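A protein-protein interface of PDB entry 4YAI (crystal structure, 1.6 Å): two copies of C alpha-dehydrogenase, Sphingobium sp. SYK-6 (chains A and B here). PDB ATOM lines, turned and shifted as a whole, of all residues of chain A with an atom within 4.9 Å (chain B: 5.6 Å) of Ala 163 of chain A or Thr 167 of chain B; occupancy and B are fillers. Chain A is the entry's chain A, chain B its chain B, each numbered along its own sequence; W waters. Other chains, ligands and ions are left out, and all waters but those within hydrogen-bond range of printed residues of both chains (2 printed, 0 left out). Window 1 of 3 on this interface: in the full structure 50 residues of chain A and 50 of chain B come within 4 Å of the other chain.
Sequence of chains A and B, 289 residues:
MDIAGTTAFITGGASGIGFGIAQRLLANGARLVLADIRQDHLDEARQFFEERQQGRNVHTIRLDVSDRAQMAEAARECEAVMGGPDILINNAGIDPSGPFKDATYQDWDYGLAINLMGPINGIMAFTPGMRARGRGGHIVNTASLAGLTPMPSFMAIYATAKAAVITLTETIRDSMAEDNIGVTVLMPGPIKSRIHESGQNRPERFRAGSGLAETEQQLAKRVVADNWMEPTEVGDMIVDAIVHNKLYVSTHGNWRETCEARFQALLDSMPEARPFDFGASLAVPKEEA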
ATOM      1  N   GLY A 147     -29.769  19.396   2.334  1.00  0.00           N
ATOM      2  CA  GLY A 147     -28.410  19.090   1.945  1.00  0.00           C
ATOM      3  C   GLY A 147     -28.277  18.901   0.449  1.00  0.00           C
ATOM      4  O   GLY A 147     -27.179  18.689  -0.049  1.00  0.00           O
ATOM      5  N   ALA A 159     -27.225  23.425   6.043  1.00  0.00           N
ATOM      6  CA  ALA A 159     -27.126  22.841   4.711  1.00  0.00           C
ATOM      7  C   ALA A 159     -25.760  22.219   4.470  1.00  0.00           C
ATOM      8  O   ALA A 159     -25.649  21.141   3.883  1.00  0.00           O
ATOM      9  CB  ALA A 159     -27.407  23.891   3.660  1.00  0.00           C
ATOM     10  N   THR A 160     -24.720  22.925   4.894  1.00  0.00           N
ATOM     11  CA  THR A 160     -23.351  22.474   4.688  1.00  0.00           C
ATOM     12  C   THR A 160     -23.131  21.118   5.366  1.00  0.00           C
ATOM     13  O   THR A 160     -22.589  20.185   4.763  1.00  0.00           O
ATOM     14  CB  THR A 160     -22.338  23.531   5.216  1.00  0.00           C
ATOM     15  OG1 THR A 160     -22.489  24.755   4.486  1.00  0.00           O
ATOM     16  CG2 THR A 160     -20.899  23.061   5.092  1.00  0.00           C
ATOM     17  N   ALA A 161     -23.567  20.992   6.612  1.00  0.00           N
ATOM     18  CA  ALA A 161     -23.421  19.729   7.334  1.00  0.00           C
ATOM     19  C   ALA A 161     -24.242  18.614   6.699  1.00  0.00           C
ATOM     20  O   ALA A 161     -23.782  17.481   6.582  1.00  0.00           O
ATOM     21  CB  ALA A 161     -23.824  19.906   8.781  1.00  0.00           C
ATOM     22  N   LYS A 162     -25.473  18.917   6.328  1.00  0.00           N
ATOM     23  CA  LYS A 162     -26.347  17.895   5.778  1.00  0.00           C
ATOM     24  C   LYS A 162     -25.871  17.380   4.410  1.00  0.00           C
ATOM     25  O   LYS A 162     -26.003  16.191   4.127  1.00  0.00           O
ATOM     26  CB  LYS A 162     -27.771  18.417   5.705  1.00  0.00           C
ATOM     27  CG  LYS A 162     -28.386  18.675   7.090  1.00  0.00           C
ATOM     28  CD  LYS A 162     -28.430  17.416   7.941  1.00  0.00           C
ATOM     29  CE  LYS A 162     -29.345  17.551   9.147  1.00  0.00           C
ATOM     30  NZ  LYS A 162     -29.474  16.272   9.890  1.00  0.00           N
ATOM     31  N   ALA A 163     -25.334  18.258   3.563  1.00  0.00           N
ATOM     32  CA  ALA A 163     -24.742  17.811   2.298  1.00  0.00           C
ATOM     33  C   ALA A 163     -23.603  16.829   2.566  1.00  0.00           C
ATOM     34  O   ALA A 163     -23.470  15.807   1.893  1.00  0.00           O
ATOM     35  CB  ALA A 163     -24.237  18.999   1.474  1.00  0.00           C
ATOM     36  N   ALA A 164     -22.780  17.148   3.557  1.00  0.00           N
ATOM     37  CA  ALA A 164     -21.679  16.279   3.961  1.00  0.00           C
ATOM     38  C   ALA A 164     -22.165  14.901   4.397  1.00  0.00           C
ATOM     39  O   ALA A 164     -21.520  13.902   4.102  1.00  0.00           O
ATOM     40  CB  ALA A 164     -20.890  16.924   5.073  1.00  0.00           C
ATOM     41  N   VAL A 165     -23.280  14.847   5.113  1.00  0.00           N
ATOM     42  CA  VAL A 165     -23.794  13.576   5.605  1.00  0.00           C
ATOM     43  C   VAL A 165     -24.253  12.688   4.440  1.00  0.00           C
ATOM     44  O   VAL A 165     -24.081  11.465   4.468  1.00  0.00           O
ATOM     45  CB  VAL A 165     -24.959  13.798   6.605  1.00  0.00           C
ATOM     46  CG1 VAL A 165     -25.635  12.479   6.961  1.00  0.00           C
ATOM     47  CG2 VAL A 165     -24.456  14.496   7.850  1.00  0.00           C
ATOM     48  N   ILE A 166     -24.842  13.300   3.415  1.00  0.00           N
ATOM     49  CA  ILE A 166     -25.232  12.553   2.227  1.00  0.00           C
ATOM     50  C   ILE A 166     -24.004  11.886   1.591  1.00  0.00           C
ATOM     51  O   ILE A 166     -23.987  10.673   1.358  1.00  0.00           O
ATOM     52  CB  ILE A 166     -25.942  13.465   1.204  1.00  0.00           C
ATOM     53  CG1 ILE A 166     -27.256  13.978   1.790  1.00  0.00           C
ATOM     54  CG2 ILE A 166     -26.203  12.710  -0.103  1.00  0.00           C
ATOM     55  CD1 ILE A 166     -27.903  15.084   1.009  1.00  0.00           C
ATOM     56  N   THR A 167     -22.968  12.678   1.340  1.00  0.00           N
ATOM     57  CA  THR A 167     -21.754  12.180   0.704  1.00  0.00           C
ATOM     58  C   THR A 167     -21.054  11.169   1.597  1.00  0.00           C
ATOM     59  O   THR A 167     -20.585  10.148   1.126  1.00  0.00           O
ATOM     60  CB  THR A 167     -20.813  13.346   0.363  1.00  0.00           C
ATOM     61  OG1 THR A 167     -21.483  14.230  -0.542  1.00  0.00           O
ATOM     62  CG2 THR A 167     -19.509  12.867  -0.270  1.00  0.00           C
ATOM     63  N   ARG A 262     -30.620  22.761  -9.961  1.00  0.00           N
ATOM     64  CA  ARG A 262     -29.267  22.748  -9.409  1.00  0.00           C
ATOM     65  C   ARG A 262     -28.370  21.759 -10.162  1.00  0.00           C
ATOM     66  O   ARG A 262     -27.264  22.100 -10.593  1.00  0.00           O
ATOM     67  CB  ARG A 262     -29.297  22.388  -7.919  1.00  0.00           C
ATOM     68  CG  ARG A 262     -27.925  22.381  -7.277  1.00  0.00           C
ATOM     69  CD  ARG A 262     -27.894  21.719  -5.918  1.00  0.00           C
ATOM     70  NE  ARG A 262     -26.508  21.665  -5.481  1.00  0.00           N
ATOM     71  CZ  ARG A 262     -25.956  20.699  -4.759  1.00  0.00           C
ATOM     72  NH1 ARG A 262     -26.679  19.683  -4.319  1.00  0.00           N
ATOM     73  NH2 ARG A 262     -24.670  20.761  -4.471  1.00  0.00           N
ATOM     74  N   LYS B 162     -15.292  17.927   0.627  1.00  0.00           N
ATOM     75  CA  LYS B 162     -15.445  18.676  -0.614  1.00  0.00           C
ATOM     76  C   LYS B 162     -16.912  18.897  -0.984  1.00  0.00           C
ATOM     77  O   LYS B 162     -17.261  19.935  -1.525  1.00  0.00           O
ATOM     78  CB  LYS B 162     -14.715  17.964  -1.751  1.00  0.00           C
ATOM     79  CG  LYS B 162     -13.182  17.937  -1.588  1.00  0.00           C
ATOM     80  CD  LYS B 162     -12.571  19.331  -1.542  1.00  0.00           C
ATOM     81  CE  LYS B 162     -11.053  19.320  -1.666  1.00  0.00           C
ATOM     82  NZ  LYS B 162     -10.531  20.704  -1.780  1.00  0.00           N
ATOM     83  N   ALA B 163     -17.776  17.922  -0.708  1.00  0.00           N
ATOM     84  CA  ALA B 163     -19.209  18.113  -0.922  1.00  0.00           C
ATOM     85  C   ALA B 163     -19.710  19.277  -0.066  1.00  0.00           C
ATOM     86  O   ALA B 163     -20.499  20.108  -0.527  1.00  0.00           O
ATOM     87  CB  ALA B 163     -19.981  16.843  -0.600  1.00  0.00           C
ATOM     88  N   ALA B 164     -19.219  19.356   1.166  1.00  0.00           N
ATOM     89  CA  ALA B 164     -19.613  20.426   2.070  1.00  0.00           C
ATOM     90  C   ALA B 164     -19.165  21.797   1.549  1.00  0.00           C
ATOM     91  O   ALA B 164     -19.871  22.784   1.714  1.00  0.00           O
ATOM     92  CB  ALA B 164     -19.052  20.173   3.456  1.00  0.00           C
ATOM     93  N   VAL B 165     -17.998  21.854   0.920  1.00  0.00           N
ATOM     94  CA  VAL B 165     -17.486  23.112   0.386  1.00  0.00           C
ATOM     95  C   VAL B 165     -18.355  23.603  -0.774  1.00  0.00           C
ATOM     96  O   VAL B 165     -18.562  24.808  -0.926  1.00  0.00           O
ATOM     97  CB  VAL B 165     -16.013  22.978  -0.064  1.00  0.00           C
ATOM     98  CG1 VAL B 165     -15.540  24.219  -0.823  1.00  0.00           C
ATOM     99  CG2 VAL B 165     -15.124  22.728   1.148  1.00  0.00           C
ATOM    100  N   ILE B 166     -18.864  22.684  -1.595  1.00  0.00           N
ATOM    101  CA  ILE B 166     -19.761  23.080  -2.686  1.00  0.00           C
ATOM    102  C   ILE B 166     -21.009  23.735  -2.096  1.00  0.00           C
ATOM    103  O   ILE B 166     -21.412  24.829  -2.509  1.00  0.00           O
ATOM    104  CB  ILE B 166     -20.145  21.866  -3.574  1.00  0.00           C
ATOM    105  CG1 ILE B 166     -18.906  21.370  -4.319  1.00  0.00           C
ATOM    106  CG2 ILE B 166     -21.267  22.222  -4.567  1.00  0.00           C
ATOM    107  CD1 ILE B 166     -19.071  20.022  -4.985  1.00  0.00           C
ATOM    108  N   THR B 167     -21.625  23.061  -1.133  1.00  0.00           N
ATOM    109  CA  THR B 167     -22.862  23.551  -0.520  1.00  0.00           C
ATOM    110  C   THR B 167     -22.629  24.842   0.265  1.00  0.00           C
ATOM    111  O   THR B 167     -23.457  25.762   0.233  1.00  0.00           O
ATOM    112  CB  THR B 167     -23.469  22.471   0.398  1.00  0.00           C
ATOM    113  OG1 THR B 167     -23.743  21.304  -0.379  1.00  0.00           O
ATOM    114  CG2 THR B 167     -24.742  22.959   1.068  1.00  0.00           C
ATOM    115  N   LEU B 168     -21.511  24.915   0.972  1.00  0.00           N
ATOM    116  CA  LEU B 168     -21.114  26.135   1.660  1.00  0.00           C
ATOM    117  C   LEU B 168     -21.131  27.324   0.710  1.00  0.00           C
ATOM    118  O   LEU B 168     -21.695  28.373   1.008  1.00  0.00           O
ATOM    119  CB  LEU B 168     -19.716  25.969   2.252  1.00  0.00           C
ATOM    120  CG  LEU B 168     -19.002  27.216   2.782  1.00  0.00           C
ATOM    121  CD1 LEU B 168     -19.692  27.745   4.030  1.00  0.00           C
ATOM    122  CD2 LEU B 168     -17.551  26.898   3.051  1.00  0.00           C
ATOM    123  N   THR B 169     -20.496  27.146  -0.437  1.00  0.00           N
ATOM    124  CA  THR B 169     -20.383  28.212  -1.420  1.00  0.00           C
ATOM    125  C   THR B 169     -21.752  28.613  -1.971  1.00  0.00           C
ATOM    126  O   THR B 169     -22.058  29.805  -2.075  1.00  0.00           O
ATOM    127  CB  THR B 169     -19.462  27.802  -2.582  1.00  0.00           C
ATOM    128  OG1 THR B 169     -18.226  27.310  -2.059  1.00  0.00           O
ATOM    129  CG2 THR B 169     -19.169  28.994  -3.468  1.00  0.00           C
ATOM    130  N   GLU B 170     -22.584  27.633  -2.309  1.00  0.00           N
ATOM    131  CA  GLU B 170     -23.942  27.921  -2.756  1.00  0.00           C
ATOM    132  C   GLU B 170     -24.724  28.739  -1.735  1.00  0.00           C
ATOM    133  O   GLU B 170     -25.401  29.709  -2.091  1.00  0.00           O
ATOM    134  CB  GLU B 170     -24.700  26.624  -3.036  1.00  0.00           C
ATOM    135  CG  GLU B 170     -24.128  25.804  -4.164  1.00  0.00           C
ATOM    136  CD  GLU B 170     -24.756  24.422  -4.247  1.00  0.00           C
ATOM    137  OE1 GLU B 170     -25.409  24.003  -3.266  1.00  0.00           O
ATOM    138  OE2 GLU B 170     -24.597  23.755  -5.289  1.00  0.00           O
ATOM    139  N   THR B 171     -24.648  28.351  -0.465  1.00  0.00           N
ATOM    140  CA  THR B 171     -25.519  28.957   0.537  1.00  0.00           C
ATOM    141  C   THR B 171     -25.085  30.361   0.905  1.00  0.00           C
ATOM    142  O   THR B 171     -25.930  31.201   1.179  1.00  0.00           O
ATOM    143  CB  THR B 171     -25.613  28.098   1.824  1.00  0.00           C
ATOM    144  OG1 THR B 171     -24.328  27.999   2.463  1.00  0.00           O
ATOM    145  CG2 THR B 171     -26.144  26.730   1.477  1.00  0.00           C
ATOM    146  N   ILE B 172     -23.786  30.646   0.893  1.00  0.00           N
ATOM    147  CA  ILE B 172     -23.353  31.987   1.297  1.00  0.00           C
ATOM    148  C   ILE B 172     -23.569  33.030   0.206  1.00  0.00           C
ATOM    149  O   ILE B 172     -23.445  34.226   0.467  1.00  0.00           O
ATOM    150  CB  ILE B 172     -21.862  32.040   1.726  1.00  0.00           C
ATOM    151  CG1 ILE B 172     -20.928  31.717   0.554  1.00  0.00           C
ATOM    152  CG2 ILE B 172     -21.639  31.121   2.932  1.00  0.00           C
ATOM    153  CD1 ILE B 172     -19.424  31.793   0.903  1.00  0.00           C
HETATM  154  O   HOH W   1     -26.074  21.653  -1.788  1.00  0.00           O
HETATM  155  O   HOH W   2     -23.013  19.363  -2.448  1.00  0.00           O
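Ala 163 of chain A touches Thr 167 of chain B, and with the chains exchanged Thr 167 of chain A touches Ala 163 of chain B.
Of the 9 pairs that touch across the chains among the printed residues, 2 have their exchanged pair printed and touching as well.
Of the 11 printed residues of chain B, 7 touch a printed residue of chain A.
Printed residues of chain B that touch a printed residue of chain A: Ala 163, Ala 164, Ile 166, Thr 167, Leu 168, Glu 170 and Thr 171.
Hydrophobic or aromatic side chains of chain B that line the printed part of chain A: Ala 163, Ala 164, Ile 166 and Leu 168.
Along chain B the printed residues that touch a printed residue of chain A span positions 163 to 171.
Printed residues of chain A that touch a printed residue of chain B: Ala 159, Thr 160, Ala 163, Thr 167 and Arg 262.
Hydrophobic or aromatic side chains of chain A that line the printed part of chain B: Ala 159 and Ala 163.
Among the printed residues, 9 pairs touch across the chains.
Among the printed residues, Asp or Glu carboxylates within 4 Å of a Lys or Arg side-chain nitrogen of the other chain: Arg 262 of chain A with Glu 170 of chain B (2.8 Å).
O of Ala 159 of chain A touches CG2 of Thr 167 of chain B, at 3.5 Å.
CB of Ala 159 of chain A touches CG2 of Thr 171 of chain B, 3.8 Å away.
Ala 164 of chain B touches Thr 160 of chain A (O to CG2, 3.5 Å).
N of Thr 160 of chain A touches CG2 of Thr 167 of chain B, at 3.8 Å.
Thr 160 of chain A touches Leu 168 of chain B (OG1 to CA, 3.4 Å).
Ala 163 of chain A touches Thr 167 of chain B (CB to OG1, 3.0 Å).
Thr 167 of chain A touches Ala 163 of chain B (OG1 to CB, 3.0 Å).
NH2 of Arg 262 of chain A touches CG2 of Ile 166 of chain B, at 3.7 Å.
OE2 of Glu 170 of chain B lies within salt-bridge range of NE of Arg 262 of chain A (2.8 Å).
Ala 163 of chain A touches just one residue of chain B: Thr 167 (3.0 Å).
Of chain A, only Ala 159, Thr 160 and Ala 163 come within 4 Å of Thr 167 of chain B.
Of the printed residues of chain B, Ala 159 of chain A touches Thr 167 and Thr 171.
Printed residues of chain A within 4 Å of Ala 163 of chain B: Thr 167.
Of the printed residues of chain A, Ala 164 of chain B touches Thr 160 (3.5 Å).
Printed residues of chain B within 4 Å of Thr 160 of chain A: Ala 164, Thr 167 and Leu 168.
Printed residues of chain A within 4 Å of Ile 166 of chain B: Arg 262 (3.7 Å).
Lys 162 of chain B touches none of the printed residues of chain A.
Ala 161 of chain A touches none of the printed residues of chain B.
The nearest residue of chain A that does not touch Thr 167 of chain B is Arg 262 of chain A (4.2 Å).
The nearest printed residue of chain B that does not touch Thr 160 of chain A is Thr 171 of chain B (4.2 Å).
The backbone carbonyl oxygen of Ala 163 of chain B is in hydrogen-bond range of the side-chain hydroxyl of Thr 167 of chain B (3.5 Å).
The backbone carbonyl oxygen (O) of Thr 167 of chain B lies close to the side-chain hydroxyl (OG1) of Thr 171 of chain B (3.3 Å).
O of Leu 168 of chain B is in hydrogen-bond range of OG1 of Thr 171 of chain B (3.0 Å).
Water W1 lies within hydrogen-bond range of the side-chain hydroxyl (OG1) of Thr 167 of chain B, the side-chain carboxylate (OE1) of Glu 170 of chain B and the guanidinium group (NH2) of Arg 262 of chain A.
Water W2 lies within hydrogen-bond range of OG1 of Thr 167 of chain B (2.9 Å), NH2 of Arg 262 of chain A (3.0 Å) and O of Ala 163 of chain B (3.3 Å).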
